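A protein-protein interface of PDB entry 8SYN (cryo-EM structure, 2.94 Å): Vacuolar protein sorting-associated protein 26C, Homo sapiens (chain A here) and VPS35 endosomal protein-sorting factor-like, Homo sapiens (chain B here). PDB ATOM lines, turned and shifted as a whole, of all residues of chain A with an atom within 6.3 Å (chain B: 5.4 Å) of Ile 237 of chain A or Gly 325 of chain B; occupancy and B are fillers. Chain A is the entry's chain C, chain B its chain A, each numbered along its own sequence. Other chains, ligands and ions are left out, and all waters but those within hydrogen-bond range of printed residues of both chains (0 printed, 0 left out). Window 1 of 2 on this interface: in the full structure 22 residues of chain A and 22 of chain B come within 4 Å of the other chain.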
ATOM      1  N   LEU A 197      14.050  -2.491 -15.069  1.00  0.00           N
ATOM      2  CA  LEU A 197      15.137  -2.157 -15.981  1.00  0.00           C
ATOM      3  C   LEU A 197      15.829  -3.445 -16.392  1.00  0.00           C
ATOM      4  O   LEU A 197      16.298  -4.197 -15.535  1.00  0.00           O
ATOM      5  CB  LEU A 197      16.130  -1.195 -15.330  1.00  0.00           C
ATOM      6  CG  LEU A 197      17.244  -0.686 -16.241  1.00  0.00           C
ATOM      7  CD1 LEU A 197      16.694   0.298 -17.252  1.00  0.00           C
ATOM      8  CD2 LEU A 197      18.344  -0.051 -15.426  1.00  0.00           C
ATOM      9  N   SER A 208      27.592   0.163 -12.157  1.00  0.00           N
ATOM     10  CA  SER A 208      26.520   0.591 -11.270  1.00  0.00           C
ATOM     11  C   SER A 208      25.427   1.276 -12.073  1.00  0.00           C
ATOM     12  O   SER A 208      25.714   2.035 -13.001  1.00  0.00           O
ATOM     13  CB  SER A 208      27.044   1.541 -10.188  1.00  0.00           C
ATOM     14  OG  SER A 208      25.995   1.982  -9.345  1.00  0.00           O
ATOM     15  N   VAL A 209      24.178   0.998 -11.707  1.00  0.00           N
ATOM     16  CA  VAL A 209      23.010   1.706 -12.213  1.00  0.00           C
ATOM     17  C   VAL A 209      22.266   2.265 -11.010  1.00  0.00           C
ATOM     18  O   VAL A 209      21.874   1.504 -10.115  1.00  0.00           O
ATOM     19  CB  VAL A 209      22.084   0.801 -13.039  1.00  0.00           C
ATOM     20  CG1 VAL A 209      21.019   1.633 -13.722  1.00  0.00           C
ATOM     21  CG2 VAL A 209      22.879   0.014 -14.055  1.00  0.00           C
ATOM     22  N   GLU A 210      22.071   3.581 -10.988  1.00  0.00           N
ATOM     23  CA  GLU A 210      21.488   4.250  -9.837  1.00  0.00           C
ATOM     24  C   GLU A 210      20.472   5.287 -10.288  1.00  0.00           C
ATOM     25  O   GLU A 210      20.592   5.877 -11.364  1.00  0.00           O
ATOM     26  CB  GLU A 210      22.572   4.907  -8.971  1.00  0.00           C
ATOM     27  CG  GLU A 210      23.311   6.040  -9.648  1.00  0.00           C
ATOM     28  CD  GLU A 210      24.414   6.616  -8.785  1.00  0.00           C
ATOM     29  OE1 GLU A 210      24.618   6.112  -7.661  1.00  0.00           O
ATOM     30  OE2 GLU A 210      25.081   7.573  -9.234  1.00  0.00           O
ATOM     31  N   LEU A 211      19.463   5.493  -9.449  1.00  0.00           N
ATOM     32  CA  LEU A 211      18.468   6.534  -9.643  1.00  0.00           C
ATOM     33  C   LEU A 211      18.929   7.814  -8.963  1.00  0.00           C
ATOM     34  O   LEU A 211      19.648   7.783  -7.962  1.00  0.00           O
ATOM     35  CB  LEU A 211      17.117   6.099  -9.079  1.00  0.00           C
ATOM     36  CG  LEU A 211      16.430   4.914  -9.755  1.00  0.00           C
ATOM     37  CD1 LEU A 211      15.434   4.290  -8.807  1.00  0.00           C
ATOM     38  CD2 LEU A 211      15.731   5.375 -11.003  1.00  0.00           C
ATOM     39  N   ILE A 235      19.976   6.667  -5.258  1.00  0.00           N
ATOM     40  CA  ILE A 235      19.623   5.332  -4.794  1.00  0.00           C
ATOM     41  C   ILE A 235      20.090   4.335  -5.844  1.00  0.00           C
ATOM     42  O   ILE A 235      19.486   4.214  -6.915  1.00  0.00           O
ATOM     43  CB  ILE A 235      18.127   5.186  -4.505  1.00  0.00           C
ATOM     44  CG1 ILE A 235      17.729   6.119  -3.361  1.00  0.00           C
ATOM     45  CG2 ILE A 235      17.771   3.757  -4.192  1.00  0.00           C
ATOM     46  CD1 ILE A 235      16.253   6.244  -3.158  1.00  0.00           C
ATOM     47  N   GLN A 236      21.174   3.625  -5.543  1.00  0.00           N
ATOM     48  CA  GLN A 236      21.694   2.610  -6.443  1.00  0.00           C
ATOM     49  C   GLN A 236      20.763   1.409  -6.479  1.00  0.00           C
ATOM     50  O   GLN A 236      20.308   0.924  -5.440  1.00  0.00           O
ATOM     51  CB  GLN A 236      23.089   2.181  -5.996  1.00  0.00           C
ATOM     52  CG  GLN A 236      23.840   1.327  -6.989  1.00  0.00           C
ATOM     53  CD  GLN A 236      25.083   0.716  -6.384  1.00  0.00           C
ATOM     54  OE1 GLN A 236      25.197   0.604  -5.166  1.00  0.00           O
ATOM     55  NE2 GLN A 236      26.026   0.328  -7.229  1.00  0.00           N
ATOM     56  N   ILE A 237      20.479   0.926  -7.684  1.00  0.00           N
ATOM     57  CA  ILE A 237      19.615  -0.232  -7.857  1.00  0.00           C
ATOM     58  C   ILE A 237      20.335  -1.432  -8.450  1.00  0.00           C
ATOM     59  O   ILE A 237      19.876  -2.568  -8.248  1.00  0.00           O
ATOM     60  CB  ILE A 237      18.380   0.117  -8.712  1.00  0.00           C
ATOM     61  CG1 ILE A 237      18.814   0.693 -10.057  1.00  0.00           C
ATOM     62  CG2 ILE A 237      17.484   1.092  -7.976  1.00  0.00           C
ATOM     63  CD1 ILE A 237      17.718   0.753 -11.077  1.00  0.00           C
ATOM     64  N   ALA A 238      21.435  -1.246  -9.175  1.00  0.00           N
ATOM     65  CA  ALA A 238      22.187  -2.359  -9.741  1.00  0.00           C
ATOM     66  C   ALA A 238      23.659  -2.170  -9.418  1.00  0.00           C
ATOM     67  O   ALA A 238      24.245  -1.148  -9.782  1.00  0.00           O
ATOM     68  CB  ALA A 238      21.975  -2.457 -11.253  1.00  0.00           C
ATOM     69  N   ASP A 239      24.251  -3.153  -8.746  1.00  0.00           N
ATOM     70  CA  ASP A 239      25.656  -3.122  -8.365  1.00  0.00           C
ATOM     71  C   ASP A 239      26.377  -4.284  -9.028  1.00  0.00           C
ATOM     72  O   ASP A 239      25.949  -5.437  -8.901  1.00  0.00           O
ATOM     73  CB  ASP A 239      25.817  -3.199  -6.847  1.00  0.00           C
ATOM     74  CG  ASP A 239      27.251  -3.003  -6.401  1.00  0.00           C
ATOM     75  OD1 ASP A 239      28.063  -2.494  -7.202  1.00  0.00           O
ATOM     76  OD2 ASP A 239      27.568  -3.358  -5.246  1.00  0.00           O
ATOM     77  N   GLY A 240      27.465  -3.984  -9.729  1.00  0.00           N
ATOM     78  CA  GLY A 240      28.207  -5.007 -10.433  1.00  0.00           C
ATOM     79  C   GLY A 240      27.553  -5.393 -11.744  1.00  0.00           C
ATOM     80  O   GLY A 240      26.518  -4.864 -12.149  1.00  0.00           O
ATOM     81  N   ASP A 241      28.183  -6.347 -12.423  1.00  0.00           N
ATOM     82  CA  ASP A 241      27.713  -6.808 -13.727  1.00  0.00           C
ATOM     83  C   ASP A 241      26.459  -7.648 -13.533  1.00  0.00           C
ATOM     84  O   ASP A 241      26.527  -8.809 -13.128  1.00  0.00           O
ATOM     85  CB  ASP A 241      28.803  -7.599 -14.436  1.00  0.00           C
ATOM     86  CG  ASP A 241      28.630  -7.605 -15.938  1.00  0.00           C
ATOM     87  OD1 ASP A 241      27.729  -6.898 -16.433  1.00  0.00           O
ATOM     88  OD2 ASP A 241      29.395  -8.316 -16.625  1.00  0.00           O
ATOM     89  N   VAL A 242      25.306  -7.059 -13.824  1.00  0.00           N
ATOM     90  CA  VAL A 242      24.027  -7.735 -13.649  1.00  0.00           C
ATOM     91  C   VAL A 242      23.786  -8.671 -14.826  1.00  0.00           C
ATOM     92  O   VAL A 242      24.270  -8.439 -15.939  1.00  0.00           O
ATOM     93  CB  VAL A 242      22.903  -6.690 -13.501  1.00  0.00           C
ATOM     94  CG1 VAL A 242      21.551  -7.357 -13.326  1.00  0.00           C
ATOM     95  CG2 VAL A 242      23.199  -5.765 -12.339  1.00  0.00           C
ATOM     96  N   LEU A 246      17.850  -9.899 -17.020  1.00  0.00           N
ATOM     97  CA  LEU A 246      17.167  -9.953 -15.738  1.00  0.00           C
ATOM     98  C   LEU A 246      16.594  -8.584 -15.410  1.00  0.00           C
ATOM     99  O   LEU A 246      17.270  -7.563 -15.563  1.00  0.00           O
ATOM    100  CB  LEU A 246      18.120 -10.402 -14.632  1.00  0.00           C
ATOM    101  CG  LEU A 246      17.471 -11.098 -13.440  1.00  0.00           C
ATOM    102  CD1 LEU A 246      16.873 -12.422 -13.868  1.00  0.00           C
ATOM    103  CD2 LEU A 246      18.490 -11.307 -12.336  1.00  0.00           C
ATOM    104  N   VAL A 248      15.967  -5.909 -13.260  1.00  0.00           N
ATOM    105  CA  VAL A 248      16.299  -5.248 -11.995  1.00  0.00           C
ATOM    106  C   VAL A 248      15.136  -4.354 -11.584  1.00  0.00           C
ATOM    107  O   VAL A 248      14.644  -3.565 -12.412  1.00  0.00           O
ATOM    108  CB  VAL A 248      17.585  -4.440 -12.140  1.00  0.00           C
ATOM    109  CG1 VAL A 248      18.035  -3.905 -10.792  1.00  0.00           C
ATOM    110  CG2 VAL A 248      18.667  -5.287 -12.770  1.00  0.00           C
ATOM    111  N   PRO A 249      14.656  -4.439 -10.348  1.00  0.00           N
ATOM    112  CA  PRO A 249      13.506  -3.622  -9.954  1.00  0.00           C
ATOM    113  C   PRO A 249      13.878  -2.198  -9.579  1.00  0.00           C
ATOM    114  O   PRO A 249      14.598  -1.966  -8.603  1.00  0.00           O
ATOM    115  CB  PRO A 249      12.941  -4.385  -8.754  1.00  0.00           C
ATOM    116  CG  PRO A 249      14.115  -5.049  -8.159  1.00  0.00           C
ATOM    117  CD  PRO A 249      15.071  -5.361  -9.280  1.00  0.00           C
ATOM    118  N   ILE A 250      13.390  -1.237 -10.357  1.00  0.00           N
ATOM    119  CA  ILE A 250      13.507   0.167  -9.990  1.00  0.00           C
ATOM    120  C   ILE A 250      12.557   0.430  -8.832  1.00  0.00           C
ATOM    121  O   ILE A 250      11.335   0.311  -8.978  1.00  0.00           O
ATOM    122  CB  ILE A 250      13.184   1.074 -11.183  1.00  0.00           C
ATOM    123  CG1 ILE A 250      14.343   1.098 -12.174  1.00  0.00           C
ATOM    124  CG2 ILE A 250      12.872   2.483 -10.716  1.00  0.00           C
ATOM    125  CD1 ILE A 250      13.981   1.685 -13.512  1.00  0.00           C
ATOM    126  N   TYR A 251      13.114   0.777  -7.678  1.00  0.00           N
ATOM    127  CA  TYR A 251      12.316   1.088  -6.498  1.00  0.00           C
ATOM    128  C   TYR A 251      12.907   2.323  -5.848  1.00  0.00           C
ATOM    129  O   TYR A 251      14.117   2.377  -5.611  1.00  0.00           O
ATOM    130  CB  TYR A 251      12.305  -0.067  -5.507  1.00  0.00           C
ATOM    131  CG  TYR A 251      11.312   0.126  -4.394  1.00  0.00           C
ATOM    132  CD1 TYR A 251      11.730   0.287  -3.083  1.00  0.00           C
ATOM    133  CD2 TYR A 251       9.954   0.117  -4.647  1.00  0.00           C
ATOM    134  CE1 TYR A 251      10.823   0.462  -2.063  1.00  0.00           C
ATOM    135  CE2 TYR A 251       9.044   0.275  -3.636  1.00  0.00           C
ATOM    136  CZ  TYR A 251       9.479   0.454  -2.345  1.00  0.00           C
ATOM    137  OH  TYR A 251       8.567   0.619  -1.331  1.00  0.00           O
ATOM    138  N   ILE A 276      18.121   8.349 -14.470  1.00  0.00           N
ATOM    139  CA  ILE A 276      18.728   7.024 -14.475  1.00  0.00           C
ATOM    140  C   ILE A 276      20.097   7.146 -15.127  1.00  0.00           C
ATOM    141  O   ILE A 276      20.200   7.427 -16.325  1.00  0.00           O
ATOM    142  CB  ILE A 276      17.853   6.006 -15.214  1.00  0.00           C
ATOM    143  CG1 ILE A 276      16.587   5.717 -14.417  1.00  0.00           C
ATOM    144  CG2 ILE A 276      18.616   4.723 -15.441  1.00  0.00           C
ATOM    145  CD1 ILE A 276      15.591   4.868 -15.148  1.00  0.00           C
ATOM    146  N   LEU B 290      23.404  -0.253  -2.706  1.00  0.00           N
ATOM    147  CA  LEU B 290      22.323  -1.233  -2.752  1.00  0.00           C
ATOM    148  C   LEU B 290      22.460  -2.280  -1.655  1.00  0.00           C
ATOM    149  O   LEU B 290      21.490  -2.587  -0.954  1.00  0.00           O
ATOM    150  CB  LEU B 290      22.290  -1.904  -4.122  1.00  0.00           C
ATOM    151  CG  LEU B 290      21.331  -3.084  -4.247  1.00  0.00           C
ATOM    152  CD1 LEU B 290      19.916  -2.588  -4.439  1.00  0.00           C
ATOM    153  CD2 LEU B 290      21.746  -3.975  -5.394  1.00  0.00           C
ATOM    154  N   ARG B 293      21.797  -1.041   1.861  1.00  0.00           N
ATOM    155  CA  ARG B 293      20.372  -0.776   2.001  1.00  0.00           C
ATOM    156  C   ARG B 293      19.601  -2.066   2.216  1.00  0.00           C
ATOM    157  O   ARG B 293      18.776  -2.167   3.132  1.00  0.00           O
ATOM    158  CB  ARG B 293      19.850  -0.039   0.772  1.00  0.00           C
ATOM    159  CG  ARG B 293      18.373   0.262   0.829  1.00  0.00           C
ATOM    160  CD  ARG B 293      18.012   1.386  -0.111  1.00  0.00           C
ATOM    161  NE  ARG B 293      17.684   0.886  -1.438  1.00  0.00           N
ATOM    162  CZ  ARG B 293      18.465   1.012  -2.499  1.00  0.00           C
ATOM    163  NH1 ARG B 293      19.629   1.634  -2.428  1.00  0.00           N
ATOM    164  NH2 ARG B 293      18.066   0.511  -3.662  1.00  0.00           N
ATOM    165  N   CYS B 321      13.267  -9.357  -4.865  1.00  0.00           N
ATOM    166  CA  CYS B 321      13.509  -8.767  -6.178  1.00  0.00           C
ATOM    167  C   CYS B 321      14.695  -7.811  -6.155  1.00  0.00           C
ATOM    168  O   CYS B 321      15.453  -7.746  -7.129  1.00  0.00           O
ATOM    169  CB  CYS B 321      12.256  -8.050  -6.674  1.00  0.00           C
ATOM    170  SG  CYS B 321      11.007  -9.146  -7.374  1.00  0.00           S
ATOM    171  N   MET B 322      14.872  -7.072  -5.059  1.00  0.00           N
ATOM    172  CA  MET B 322      15.991  -6.146  -4.933  1.00  0.00           C
ATOM    173  C   MET B 322      17.327  -6.857  -5.033  1.00  0.00           C
ATOM    174  O   MET B 322      18.306  -6.275  -5.514  1.00  0.00           O
ATOM    175  CB  MET B 322      15.895  -5.407  -3.599  1.00  0.00           C
ATOM    176  CG  MET B 322      16.933  -4.330  -3.391  1.00  0.00           C
ATOM    177  SD  MET B 322      16.732  -3.515  -1.801  1.00  0.00           S
ATOM    178  CE  MET B 322      15.245  -2.563  -2.100  1.00  0.00           C
ATOM    179  N   ILE B 323      17.393  -8.111  -4.577  1.00  0.00           N
ATOM    180  CA  ILE B 323      18.651  -8.851  -4.641  1.00  0.00           C
ATOM    181  C   ILE B 323      19.157  -8.993  -6.077  1.00  0.00           C
ATOM    182  O   ILE B 323      20.365  -9.140  -6.293  1.00  0.00           O
ATOM    183  CB  ILE B 323      18.495 -10.229  -3.966  1.00  0.00           C
ATOM    184  CG1 ILE B 323      18.159 -10.058  -2.489  1.00  0.00           C
ATOM    185  CG2 ILE B 323      19.769 -11.035  -4.064  1.00  0.00           C
ATOM    186  CD1 ILE B 323      17.750 -11.338  -1.818  1.00  0.00           C
ATOM    187  N   ARG B 324      18.267  -8.919  -7.073  1.00  0.00           N
ATOM    188  CA  ARG B 324      18.694  -9.032  -8.466  1.00  0.00           C
ATOM    189  C   ARG B 324      19.690  -7.957  -8.870  1.00  0.00           C
ATOM    190  O   ARG B 324      20.441  -8.157  -9.829  1.00  0.00           O
ATOM    191  CB  ARG B 324      17.498  -8.968  -9.415  1.00  0.00           C
ATOM    192  CG  ARG B 324      16.559 -10.144  -9.340  1.00  0.00           C
ATOM    193  CD  ARG B 324      15.420  -9.970 -10.321  1.00  0.00           C
ATOM    194  NE  ARG B 324      14.477 -11.079 -10.269  1.00  0.00           N
ATOM    195  CZ  ARG B 324      13.365 -11.148 -10.985  1.00  0.00           C
ATOM    196  NH1 ARG B 324      13.021 -10.181 -11.820  1.00  0.00           N
ATOM    197  NH2 ARG B 324      12.580 -12.214 -10.864  1.00  0.00           N
ATOM    198  N   GLY B 325      19.716  -6.822  -8.172  1.00  0.00           N
ATOM    199  CA  GLY B 325      20.662  -5.779  -8.519  1.00  0.00           C
ATOM    200  C   GLY B 325      22.099  -6.158  -8.229  1.00  0.00           C
ATOM    201  O   GLY B 325      23.020  -5.629  -8.856  1.00  0.00           O
ATOM    202  N   ILE B 326      22.312  -7.068  -7.283  1.00  0.00           N
ATOM    203  CA  ILE B 326      23.659  -7.488  -6.908  1.00  0.00           C
ATOM    204  C   ILE B 326      24.236  -8.320  -8.050  1.00  0.00           C
ATOM    205  O   ILE B 326      23.772  -9.431  -8.316  1.00  0.00           O
ATOM    206  CB  ILE B 326      23.655  -8.273  -5.594  1.00  0.00           C
ATOM    207  CG1 ILE B 326      22.984  -7.453  -4.494  1.00  0.00           C
ATOM    208  CG2 ILE B 326      25.070  -8.633  -5.194  1.00  0.00           C
ATOM    209  CD1 ILE B 326      22.918  -8.155  -3.167  1.00  0.00           C
ATOM    210  N   GLY B 327      25.255  -7.783  -8.724  1.00  0.00           N
ATOM    211  CA  GLY B 327      25.816  -8.470  -9.873  1.00  0.00           C
ATOM    212  C   GLY B 327      26.830  -9.538  -9.529  1.00  0.00           C
ATOM    213  O   GLY B 327      27.008 -10.489 -10.296  1.00  0.00           O
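The backbone carbonyl oxygen (O) of Asp 241 of chain A lies close to the backbone carbonyl oxygen (O) of Gly 327 of chain B, at 3.3 Å.
O of Gln 236 of chain A is in hydrogen-bond range of NH2 of Arg 293 of chain B, 2.9 Å away.
The backbone carbonyl oxygen (O) of Gly 325 of chain B is in hydrogen-bond range of the backbone NH (N) of Asp 239 of chain A (2.8 Å).
OE1 of Gln 236 of chain A sits at hydrogen-bond distance from N of Leu 290 of chain B (3.2 Å).
N of Gly 327 of chain B is in hydrogen-bond range of O of Asp 239 of chain A, at 2.5 Å.
The backbone carbonyl oxygen (O) of Leu 197 of chain A sits at hydrogen-bond distance from the backbone NH (N) of Val 248 of chain A.
O of Val 209 of chain A sits at hydrogen-bond distance from N of Ile 237 of chain A.
NE2 of Gln 236 of chain A is in hydrogen-bond range of OD1 of Asp 239 of chain A, at 3.5 Å.
The backbone NH of Leu 211 of chain A lies within hydrogen-bond range of the backbone carbonyl oxygen of Ile 235 of chain A, 2.8 Å away.
NE2 of Gln 236 of chain A lies within hydrogen-bond range of OG of Ser 208 of chain A (2.7 Å).
The backbone carbonyl oxygen of Ala 238 of chain A lies within hydrogen-bond range of the backbone NH of Val 209 of chain A (2.9 Å).
Ile 235 of chain A touches Arg 293 of chain B (CG2 to CZ, 3.3 Å).
Ile 237 of chain A touches Leu 290 of chain B (O to CD2, 3.7 Å).
Gly 325 of chain B touches Ala 238 of chain A.
Ile 326 of chain B touches Asp 239 of chain A (C to O, 3.5 Å).
Gly 240 of chain A touches Gly 327 of chain B.
Arg 324 of chain B touches Val 242 of chain A (O to CG1, 3.8 Å).
O of Gly 325 of chain B touches CG2 of Val 242 of chain A, at 3.5 Å.
CD2 of Leu 246 of chain A touches CG of Arg 324 of chain B, 3.7 Å away.
Cys 321 of chain B touches Pro 249 of chain A.
Met 322 of chain B touches Pro 249 of chain A (N to CG, 3.8 Å).
Of the printed residues of chain B, Gln 236 of chain A touches Leu 290 (3.2 Å) and Arg 293 (2.9 Å).
Of chain B, only Leu 290 and Gly 325 come within 4 Å of Ile 237 of chain A.
Printed residues of chain B within 4 Å of Asp 241 of chain A: Gly 327 (3.3 Å).
Of the printed residues of chain B, Leu 246 of chain A touches Arg 324.
Printed residues of chain B within 4 Å of Pro 249 of chain A: Cys 321 and Met 322.
Tyr 251 of chain A touches none of the printed residues of chain B.
Ile 276 of chain A touches none of the printed residues of chain B.
Gly 325 of chain B touches five residues of chain A.
Of the printed residues of chain A, Ile 326 of chain B touches Asp 239 (3.5 Å).
The nearest residue of chain B that does not touch Ile 237 of chain A is Arg 293 of chain B (4.4 Å).
The nearest residue of chain A that does not touch Gly 325 of chain B is Gly 240 of chain A (4.8 Å).
Printed residues of chain A that touch a printed residue of chain B: Ile 235, Gln 236, Ile 237, Ala 238, Asp 239, Gly 240, Asp 241, Val 242, Leu 246, Val 248 and Pro 249.
Hydrophobic or aromatic side chains of chain B that line the printed part of chain A: Leu 290.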
